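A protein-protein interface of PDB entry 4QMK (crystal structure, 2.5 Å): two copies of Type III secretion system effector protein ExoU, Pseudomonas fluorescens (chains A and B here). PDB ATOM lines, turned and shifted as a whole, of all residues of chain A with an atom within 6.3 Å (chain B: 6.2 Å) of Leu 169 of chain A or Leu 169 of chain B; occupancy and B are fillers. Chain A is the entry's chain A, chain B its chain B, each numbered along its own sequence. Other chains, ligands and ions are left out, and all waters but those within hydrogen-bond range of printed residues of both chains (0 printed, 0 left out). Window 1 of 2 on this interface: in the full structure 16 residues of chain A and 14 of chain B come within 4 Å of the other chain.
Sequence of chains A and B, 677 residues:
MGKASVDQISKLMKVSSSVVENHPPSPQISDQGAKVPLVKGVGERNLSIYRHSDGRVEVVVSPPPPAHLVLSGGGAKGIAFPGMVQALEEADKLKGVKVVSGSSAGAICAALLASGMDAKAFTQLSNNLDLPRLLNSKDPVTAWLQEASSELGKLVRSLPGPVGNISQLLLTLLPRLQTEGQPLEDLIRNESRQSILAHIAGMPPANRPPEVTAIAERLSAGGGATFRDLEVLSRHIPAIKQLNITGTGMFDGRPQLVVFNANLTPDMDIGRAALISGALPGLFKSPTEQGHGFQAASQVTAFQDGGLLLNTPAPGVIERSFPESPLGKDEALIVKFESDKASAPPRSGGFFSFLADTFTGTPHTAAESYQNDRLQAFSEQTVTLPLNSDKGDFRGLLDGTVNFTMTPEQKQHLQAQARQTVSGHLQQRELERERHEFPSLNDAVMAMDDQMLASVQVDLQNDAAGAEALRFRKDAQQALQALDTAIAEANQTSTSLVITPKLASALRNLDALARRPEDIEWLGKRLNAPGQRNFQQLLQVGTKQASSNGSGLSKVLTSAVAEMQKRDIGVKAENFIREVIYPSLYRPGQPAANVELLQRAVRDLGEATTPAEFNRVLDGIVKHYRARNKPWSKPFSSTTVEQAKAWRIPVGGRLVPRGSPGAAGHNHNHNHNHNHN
The side-chain hydroxyl (OG1) of Thr 172 of chain A lies within hydrogen-bond range of the backbone carbonyl oxygen (O) of Leu 169 of chain A (3.4 Å).
O of Leu 169 of chain B lies within hydrogen-bond range of OG1 of Thr 172 of chain B, at 3.5 Å.
Among the printed residues, merely in contact across the chains: Leu 155 of chain A with Leu 155 of chain B (3.5 Å), Val 163 of chain A with Thr 172 of chain B (3.7 Å), Leu 169 of chain A with Leu 169 of chain B (3.5 Å), Leu 169 of chain A with Leu 173 of chain B (3.6 Å), Thr 172 of chain A with Thr 172 of chain B (3.5 Å), Leu 173 of chain A with Leu 155 of chain B (3.5 Å) and Leu 173 of chain A with Leu 169 of chain B (3.6 Å).
Of the printed residues of chain B, Leu 155 of chain A touches Leu 155 (3.5 Å).
Of chain B, only Leu 169 and Leu 173 come within 4 Å of Leu 169 of chain A.
Of the printed residues of chain A, Leu 155 of chain B touches Leu 155 (3.5 Å) and Leu 173 (3.5 Å).
Leu 169 of chain B touches just these residues of chain A: Leu 169 (3.5 Å) and Leu 173 (3.6 Å).
Printed residues of chain A within 4 Å of Thr 172 of chain B: Val 163 (3.7 Å) and Thr 172 (3.5 Å).
Of the 14 printed residues of chain B, 4 touch a printed residue of chain A.
Printed residues of chain B that touch a printed residue of chain A: Leu 155, Leu 169, Thr 172 and Leu 173.
Printed residues of chain A that touch a printed residue of chain B: Leu 155, Val 163, Leu 169, Thr 172 and Leu 173.
Val 163 of chain A touches Thr 172 of chain B, but with the chains exchanged Thr 172 of chain A does not touch Val 163 of chain B (4.1 Å).
Leu 169 of chain A touches its own counterpart, Leu 169 of chain B.
Leu 169 of chain A touches Leu 173 of chain B, and with the chains exchanged Leu 173 of chain A touches Leu 169 of chain B.
Thr 172 of chain A touches its own counterpart, Thr 172 of chain B.
Positions printed for both chains: 152, 155, 156, 163, 165, 166, 167, 168, 169, 170, 171, 172, 173 and 174.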
ATOM      1  N   LEU A 152     -19.086 -19.765 -22.474  1.00  0.00           N
ATOM      2  CA  LEU A 152     -18.166 -20.778 -22.022  1.00  0.00           C
ATOM      3  C   LEU A 152     -16.739 -20.573 -22.449  1.00  0.00           C
ATOM      4  O   LEU A 152     -15.793 -20.949 -21.723  1.00  0.00           O
ATOM      5  CB  LEU A 152     -18.608 -22.151 -22.509  1.00  0.00           C
ATOM      6  CG  LEU A 152     -19.701 -22.765 -21.680  1.00  0.00           C
ATOM      7  CD1 LEU A 152     -20.184 -24.044 -22.335  1.00  0.00           C
ATOM      8  CD2 LEU A 152     -19.193 -23.027 -20.284  1.00  0.00           C
ATOM      9  N   LEU A 155     -15.243 -17.583 -20.238  1.00  0.00           N
ATOM     10  CA  LEU A 155     -15.036 -17.924 -18.859  1.00  0.00           C
ATOM     11  C   LEU A 155     -13.799 -18.769 -18.666  1.00  0.00           C
ATOM     12  O   LEU A 155     -12.857 -18.356 -17.975  1.00  0.00           O
ATOM     13  CB  LEU A 155     -16.258 -18.618 -18.313  1.00  0.00           C
ATOM     14  CG  LEU A 155     -17.467 -17.714 -18.047  1.00  0.00           C
ATOM     15  CD1 LEU A 155     -18.694 -18.582 -17.848  1.00  0.00           C
ATOM     16  CD2 LEU A 155     -17.275 -16.825 -16.835  1.00  0.00           C
ATOM     17  N   VAL A 156     -13.732 -19.882 -19.382  1.00  0.00           N
ATOM     18  CA  VAL A 156     -12.631 -20.837 -19.152  1.00  0.00           C
ATOM     19  C   VAL A 156     -11.236 -20.344 -19.516  1.00  0.00           C
ATOM     20  O   VAL A 156     -10.247 -20.720 -18.843  1.00  0.00           O
ATOM     21  CB  VAL A 156     -12.872 -22.161 -19.880  1.00  0.00           C
ATOM     22  CG1 VAL A 156     -11.735 -23.141 -19.661  1.00  0.00           C
ATOM     23  CG2 VAL A 156     -14.135 -22.776 -19.338  1.00  0.00           C
ATOM     24  N   VAL A 163      -7.685 -24.134 -15.015  1.00  0.00           N
ATOM     25  CA  VAL A 163      -8.308 -25.379 -14.664  1.00  0.00           C
ATOM     26  C   VAL A 163      -7.733 -26.410 -15.651  1.00  0.00           C
ATOM     27  O   VAL A 163      -6.967 -26.092 -16.591  1.00  0.00           O
ATOM     28  CB  VAL A 163      -9.876 -25.343 -14.808  1.00  0.00           C
ATOM     29  CG1 VAL A 163     -10.491 -24.213 -13.983  1.00  0.00           C
ATOM     30  CG2 VAL A 163     -10.324 -25.259 -16.285  1.00  0.00           C
ATOM     31  N   ASN A 165      -9.450 -28.615 -17.944  1.00  0.00           N
ATOM     32  CA  ASN A 165     -10.072 -28.743 -19.280  1.00  0.00           C
ATOM     33  C   ASN A 165     -11.500 -28.229 -19.196  1.00  0.00           C
ATOM     34  O   ASN A 165     -12.130 -28.295 -18.159  1.00  0.00           O
ATOM     35  CB  ASN A 165     -10.083 -30.202 -19.767  1.00  0.00           C
ATOM     36  CG  ASN A 165     -10.659 -30.366 -21.224  1.00  0.00           C
ATOM     37  OD1 ASN A 165     -11.855 -30.697 -21.422  1.00  0.00           O
ATOM     38  ND2 ASN A 165      -9.807 -30.186 -22.218  1.00  0.00           N
ATOM     39  N   ILE A 166     -11.998 -27.674 -20.272  1.00  0.00           N
ATOM     40  CA  ILE A 166     -13.371 -27.210 -20.284  1.00  0.00           C
ATOM     41  C   ILE A 166     -14.361 -28.339 -19.951  1.00  0.00           C
ATOM     42  O   ILE A 166     -15.446 -28.079 -19.480  1.00  0.00           O
ATOM     43  CB  ILE A 166     -13.700 -26.524 -21.602  1.00  0.00           C
ATOM     44  CG1 ILE A 166     -14.992 -25.779 -21.496  1.00  0.00           C
ATOM     45  CG2 ILE A 166     -13.769 -27.489 -22.749  1.00  0.00           C
ATOM     46  CD1 ILE A 166     -15.072 -24.786 -22.631  1.00  0.00           C
ATOM     47  N   SER A 167     -13.972 -29.595 -20.127  1.00  0.00           N
ATOM     48  CA  SER A 167     -14.785 -30.690 -19.593  1.00  0.00           C
ATOM     49  C   SER A 167     -15.157 -30.529 -18.119  1.00  0.00           C
ATOM     50  O   SER A 167     -16.235 -30.928 -17.687  1.00  0.00           O
ATOM     51  CB  SER A 167     -14.042 -32.009 -19.724  1.00  0.00           C
ATOM     52  OG  SER A 167     -12.747 -31.990 -19.148  1.00  0.00           O
ATOM     53  N   GLN A 168     -14.272 -29.957 -17.329  1.00  0.00           N
ATOM     54  CA  GLN A 168     -14.555 -29.777 -15.906  1.00  0.00           C
ATOM     55  C   GLN A 168     -15.708 -28.825 -15.641  1.00  0.00           C
ATOM     56  O   GLN A 168     -16.556 -29.063 -14.784  1.00  0.00           O
ATOM     57  CB  GLN A 168     -13.274 -29.429 -15.172  1.00  0.00           C
ATOM     58  CG  GLN A 168     -12.424 -30.685 -15.030  1.00  0.00           C
ATOM     59  CD  GLN A 168     -10.974 -30.429 -14.771  1.00  0.00           C
ATOM     60  OE1 GLN A 168     -10.452 -29.360 -15.055  1.00  0.00           O
ATOM     61  NE2 GLN A 168     -10.302 -31.429 -14.272  1.00  0.00           N
ATOM     62  N   LEU A 169     -15.782 -27.776 -16.423  1.00  0.00           N
ATOM     63  CA  LEU A 169     -16.918 -26.891 -16.359  1.00  0.00           C
ATOM     64  C   LEU A 169     -18.203 -27.568 -16.778  1.00  0.00           C
ATOM     65  O   LEU A 169     -19.196 -27.391 -16.134  1.00  0.00           O
ATOM     66  CB  LEU A 169     -16.731 -25.723 -17.283  1.00  0.00           C
ATOM     67  CG  LEU A 169     -16.560 -24.362 -16.650  1.00  0.00           C
ATOM     68  CD1 LEU A 169     -16.759 -23.309 -17.733  1.00  0.00           C
ATOM     69  CD2 LEU A 169     -17.596 -24.171 -15.549  1.00  0.00           C
ATOM     70  N   LEU A 170     -18.172 -28.324 -17.878  1.00  0.00           N
ATOM     71  CA  LEU A 170     -19.364 -28.948 -18.440  1.00  0.00           C
ATOM     72  C   LEU A 170     -19.898 -29.984 -17.511  1.00  0.00           C
ATOM     73  O   LEU A 170     -21.124 -30.113 -17.330  1.00  0.00           O
ATOM     74  CB  LEU A 170     -19.053 -29.568 -19.803  1.00  0.00           C
ATOM     75  CG  LEU A 170     -18.597 -28.540 -20.821  1.00  0.00           C
ATOM     76  CD1 LEU A 170     -18.233 -29.195 -22.126  1.00  0.00           C
ATOM     77  CD2 LEU A 170     -19.661 -27.528 -21.052  1.00  0.00           C
ATOM     78  N   LEU A 171     -18.979 -30.745 -16.926  1.00  0.00           N
ATOM     79  CA  LEU A 171     -19.341 -31.723 -15.913  1.00  0.00           C
ATOM     80  C   LEU A 171     -20.271 -31.086 -14.896  1.00  0.00           C
ATOM     81  O   LEU A 171     -21.346 -31.586 -14.671  1.00  0.00           O
ATOM     82  CB  LEU A 171     -18.084 -32.234 -15.213  1.00  0.00           C
ATOM     83  CG  LEU A 171     -18.334 -32.983 -13.910  1.00  0.00           C
ATOM     84  CD1 LEU A 171     -19.258 -34.137 -14.175  1.00  0.00           C
ATOM     85  CD2 LEU A 171     -17.030 -33.499 -13.343  1.00  0.00           C
ATOM     86  N   THR A 172     -19.880 -29.946 -14.317  1.00  0.00           N
ATOM     87  CA  THR A 172     -20.696 -29.334 -13.261  1.00  0.00           C
ATOM     88  C   THR A 172     -21.854 -28.488 -13.772  1.00  0.00           C
ATOM     89  O   THR A 172     -22.758 -28.219 -13.017  1.00  0.00           O
ATOM     90  CB  THR A 172     -19.898 -28.498 -12.246  1.00  0.00           C
ATOM     91  OG1 THR A 172     -19.670 -27.210 -12.769  1.00  0.00           O
ATOM     92  CG2 THR A 172     -18.564 -29.155 -11.842  1.00  0.00           C
ATOM     93  N   LEU A 173     -21.831 -28.069 -15.029  1.00  0.00           N
ATOM     94  CA  LEU A 173     -22.968 -27.326 -15.613  1.00  0.00           C
ATOM     95  C   LEU A 173     -24.027 -28.244 -16.211  1.00  0.00           C
ATOM     96  O   LEU A 173     -25.186 -27.858 -16.326  1.00  0.00           O
ATOM     97  CB  LEU A 173     -22.511 -26.369 -16.726  1.00  0.00           C
ATOM     98  CG  LEU A 173     -21.673 -25.185 -16.259  1.00  0.00           C
ATOM     99  CD1 LEU A 173     -21.290 -24.305 -17.426  1.00  0.00           C
ATOM    100  CD2 LEU A 173     -22.453 -24.404 -15.225  1.00  0.00           C
ATOM    101  N   LEU A 174     -23.624 -29.439 -16.619  1.00  0.00           N
ATOM    102  CA  LEU A 174     -24.552 -30.359 -17.268  1.00  0.00           C
ATOM    103  C   LEU A 174     -24.599 -31.719 -16.602  1.00  0.00           C
ATOM    104  O   LEU A 174     -24.364 -32.709 -17.255  1.00  0.00           O
ATOM    105  CB  LEU A 174     -24.153 -30.544 -18.737  1.00  0.00           C
ATOM    106  CG  LEU A 174     -24.181 -29.296 -19.618  1.00  0.00           C
ATOM    107  CD1 LEU A 174     -23.697 -29.666 -21.001  1.00  0.00           C
ATOM    108  CD2 LEU A 174     -25.574 -28.730 -19.694  1.00  0.00           C
ATOM    109  N   LEU B 152     -21.167 -14.774 -16.080  1.00  0.00           N
ATOM    110  CA  LEU B 152     -21.629 -15.763 -15.114  1.00  0.00           C
ATOM    111  C   LEU B 152     -23.137 -15.776 -14.939  1.00  0.00           C
ATOM    112  O   LEU B 152     -23.711 -16.797 -14.629  1.00  0.00           O
ATOM    113  CB  LEU B 152     -20.979 -15.514 -13.754  1.00  0.00           C
ATOM    114  CG  LEU B 152     -19.589 -16.098 -13.630  1.00  0.00           C
ATOM    115  CD1 LEU B 152     -18.932 -15.616 -12.359  1.00  0.00           C
ATOM    116  CD2 LEU B 152     -19.686 -17.608 -13.623  1.00  0.00           C
ATOM    117  N   LEU B 155     -24.773 -17.423 -18.046  1.00  0.00           N
ATOM    118  CA  LEU B 155     -24.502 -18.830 -18.038  1.00  0.00           C
ATOM    119  C   LEU B 155     -25.400 -19.598 -17.047  1.00  0.00           C
ATOM    120  O   LEU B 155     -26.079 -20.570 -17.435  1.00  0.00           O
ATOM    121  CB  LEU B 155     -23.031 -19.077 -17.733  1.00  0.00           C
ATOM    122  CG  LEU B 155     -22.556 -20.477 -18.083  1.00  0.00           C
ATOM    123  CD1 LEU B 155     -22.300 -20.556 -19.571  1.00  0.00           C
ATOM    124  CD2 LEU B 155     -21.293 -20.807 -17.315  1.00  0.00           C
ATOM    125  N   VAL B 156     -25.404 -19.170 -15.786  1.00  0.00           N
ATOM    126  CA  VAL B 156     -26.118 -19.903 -14.732  1.00  0.00           C
ATOM    127  C   VAL B 156     -27.628 -19.922 -14.921  1.00  0.00           C
ATOM    128  O   VAL B 156     -28.310 -20.864 -14.521  1.00  0.00           O
ATOM    129  CB  VAL B 156     -25.742 -19.412 -13.311  1.00  0.00           C
ATOM    130  CG1 VAL B 156     -26.583 -20.096 -12.245  1.00  0.00           C
ATOM    131  CG2 VAL B 156     -24.294 -19.744 -13.030  1.00  0.00           C
ATOM    132  N   VAL B 163     -28.871 -25.747 -11.093  1.00  0.00           N
ATOM    133  CA  VAL B 163     -27.698 -26.032 -10.278  1.00  0.00           C
ATOM    134  C   VAL B 163     -28.090 -25.713  -8.834  1.00  0.00           C
ATOM    135  O   VAL B 163     -29.118 -25.077  -8.629  1.00  0.00           O
ATOM    136  CB  VAL B 163     -26.463 -25.271 -10.774  1.00  0.00           C
ATOM    137  CG1 VAL B 163     -26.400 -23.843 -10.215  1.00  0.00           C
ATOM    138  CG2 VAL B 163     -25.199 -26.075 -10.461  1.00  0.00           C
ATOM    139  N   ASN B 165     -26.453 -23.838  -6.437  1.00  0.00           N
ATOM    140  CA  ASN B 165     -26.173 -22.458  -6.080  1.00  0.00           C
ATOM    141  C   ASN B 165     -25.036 -22.028  -6.979  1.00  0.00           C
ATOM    142  O   ASN B 165     -24.201 -22.847  -7.376  1.00  0.00           O
ATOM    143  CB  ASN B 165     -25.773 -22.342  -4.592  1.00  0.00           C
ATOM    144  CG  ASN B 165     -25.532 -20.898  -4.130  1.00  0.00           C
ATOM    145  OD1 ASN B 165     -24.391 -20.400  -4.149  1.00  0.00           O
ATOM    146  ND2 ASN B 165     -26.609 -20.211  -3.745  1.00  0.00           N
ATOM    147  N   ILE B 166     -25.006 -20.753  -7.329  1.00  0.00           N
ATOM    148  CA  ILE B 166     -23.912 -20.246  -8.150  1.00  0.00           C
ATOM    149  C   ILE B 166     -22.547 -20.493  -7.476  1.00  0.00           C
ATOM    150  O   ILE B 166     -21.531 -20.546  -8.151  1.00  0.00           O
ATOM    151  CB  ILE B 166     -24.130 -18.779  -8.529  1.00  0.00           C
ATOM    152  CG1 ILE B 166     -23.168 -18.331  -9.581  1.00  0.00           C
ATOM    153  CG2 ILE B 166     -23.997 -17.898  -7.335  1.00  0.00           C
ATOM    154  CD1 ILE B 166     -23.644 -17.042 -10.204  1.00  0.00           C
ATOM    155  N   SER B 167     -22.526 -20.707  -6.163  1.00  0.00           N
ATOM    156  CA  SER B 167     -21.272 -21.145  -5.478  1.00  0.00           C
ATOM    157  C   SER B 167     -20.630 -22.359  -6.126  1.00  0.00           C
ATOM    158  O   SER B 167     -19.412 -22.506  -6.165  1.00  0.00           O
ATOM    159  CB  SER B 167     -21.541 -21.486  -4.013  1.00  0.00           C
ATOM    160  OG  SER B 167     -22.607 -22.426  -3.870  1.00  0.00           O
ATOM    161  N   GLN B 168     -21.453 -23.266  -6.608  1.00  0.00           N
ATOM    162  CA  GLN B 168     -20.910 -24.459  -7.239  1.00  0.00           C
ATOM    163  C   GLN B 168     -20.121 -24.123  -8.506  1.00  0.00           C
ATOM    164  O   GLN B 168     -19.092 -24.722  -8.757  1.00  0.00           O
ATOM    165  CB  GLN B 168     -22.011 -25.477  -7.443  1.00  0.00           C
ATOM    166  CG  GLN B 168     -22.348 -26.112  -6.114  1.00  0.00           C
ATOM    167  CD  GLN B 168     -23.727 -26.736  -6.055  1.00  0.00           C
ATOM    168  OE1 GLN B 168     -24.626 -26.439  -6.859  1.00  0.00           O
ATOM    169  NE2 GLN B 168     -23.909 -27.602  -5.074  1.00  0.00           N
ATOM    170  N   LEU B 169     -20.601 -23.159  -9.292  1.00  0.00           N
ATOM    171  CA  LEU B 169     -19.850 -22.687 -10.425  1.00  0.00           C
ATOM    172  C   LEU B 169     -18.540 -22.059 -10.015  1.00  0.00           C
ATOM    173  O   LEU B 169     -17.529 -22.359 -10.609  1.00  0.00           O
ATOM    174  CB  LEU B 169     -20.602 -21.637 -11.220  1.00  0.00           C
ATOM    175  CG  LEU B 169     -21.016 -22.002 -12.619  1.00  0.00           C
ATOM    176  CD1 LEU B 169     -21.343 -20.715 -13.363  1.00  0.00           C
ATOM    177  CD2 LEU B 169     -19.877 -22.718 -13.346  1.00  0.00           C
ATOM    178  N   LEU B 170     -18.576 -21.203  -8.999  1.00  0.00           N
ATOM    179  CA  LEU B 170     -17.396 -20.467  -8.549  1.00  0.00           C
ATOM    180  C   LEU B 170     -16.351 -21.391  -7.974  1.00  0.00           C
ATOM    181  O   LEU B 170     -15.147 -21.242  -8.237  1.00  0.00           O
ATOM    182  CB  LEU B 170     -17.793 -19.421  -7.539  1.00  0.00           C
ATOM    183  CG  LEU B 170     -18.772 -18.411  -8.105  1.00  0.00           C
ATOM    184  CD1 LEU B 170     -19.198 -17.430  -7.058  1.00  0.00           C
ATOM    185  CD2 LEU B 170     -18.142 -17.663  -9.254  1.00  0.00           C
ATOM    186  N   LEU B 171     -16.814 -22.387  -7.237  1.00  0.00           N
ATOM    187  CA  LEU B 171     -15.931 -23.404  -6.724  1.00  0.00           C
ATOM    188  C   LEU B 171     -15.065 -23.979  -7.831  1.00  0.00           C
ATOM    189  O   LEU B 171     -13.854 -23.988  -7.712  1.00  0.00           O
ATOM    190  CB  LEU B 171     -16.742 -24.524  -6.094  1.00  0.00           C
ATOM    191  CG  LEU B 171     -15.956 -25.812  -5.821  1.00  0.00           C
ATOM    192  CD1 LEU B 171     -14.776 -25.517  -4.932  1.00  0.00           C
ATOM    193  CD2 LEU B 171     -16.847 -26.846  -5.172  1.00  0.00           C
ATOM    194  N   THR B 172     -15.672 -24.421  -8.925  1.00  0.00           N
ATOM    195  CA  THR B 172     -14.901 -25.056  -9.971  1.00  0.00           C
ATOM    196  C   THR B 172     -14.195 -24.079 -10.881  1.00  0.00           C
ATOM    197  O   THR B 172     -13.226 -24.471 -11.542  1.00  0.00           O
ATOM    198  CB  THR B 172     -15.708 -26.085 -10.834  1.00  0.00           C
ATOM    199  OG1 THR B 172     -16.442 -25.406 -11.833  1.00  0.00           O
ATOM    200  CG2 THR B 172     -16.628 -26.951 -10.007  1.00  0.00           C
ATOM    201  N   LEU B 173     -14.652 -22.821 -10.943  1.00  0.00           N
ATOM    202  CA  LEU B 173     -13.935 -21.782 -11.759  1.00  0.00           C
ATOM    203  C   LEU B 173     -12.792 -21.102 -11.018  1.00  0.00           C
ATOM    204  O   LEU B 173     -11.874 -20.602 -11.623  1.00  0.00           O
ATOM    205  CB  LEU B 173     -14.877 -20.690 -12.229  1.00  0.00           C
ATOM    206  CG  LEU B 173     -15.893 -21.144 -13.230  1.00  0.00           C
ATOM    207  CD1 LEU B 173     -16.762 -19.983 -13.657  1.00  0.00           C
ATOM    208  CD2 LEU B 173     -15.195 -21.768 -14.420  1.00  0.00           C
ATOM    209  N   LEU B 174     -12.874 -21.056  -9.699  1.00  0.00           N
ATOM    210  CA  LEU B 174     -11.865 -20.368  -8.906  1.00  0.00           C
ATOM    211  C   LEU B 174     -11.250 -21.266  -7.831  1.00  0.00           C
ATOM    212  O   LEU B 174     -11.314 -20.945  -6.655  1.00  0.00           O
ATOM    213  CB  LEU B 174     -12.503 -19.149  -8.233  1.00  0.00           C
ATOM    214  CG  LEU B 174     -13.043 -18.074  -9.148  1.00  0.00           C
ATOM    215  CD1 LEU B 174     -13.685 -16.977  -8.316  1.00  0.00           C
ATOM    216  CD2 LEU B 174     -11.945 -17.499 -10.001  1.00  0.00           C
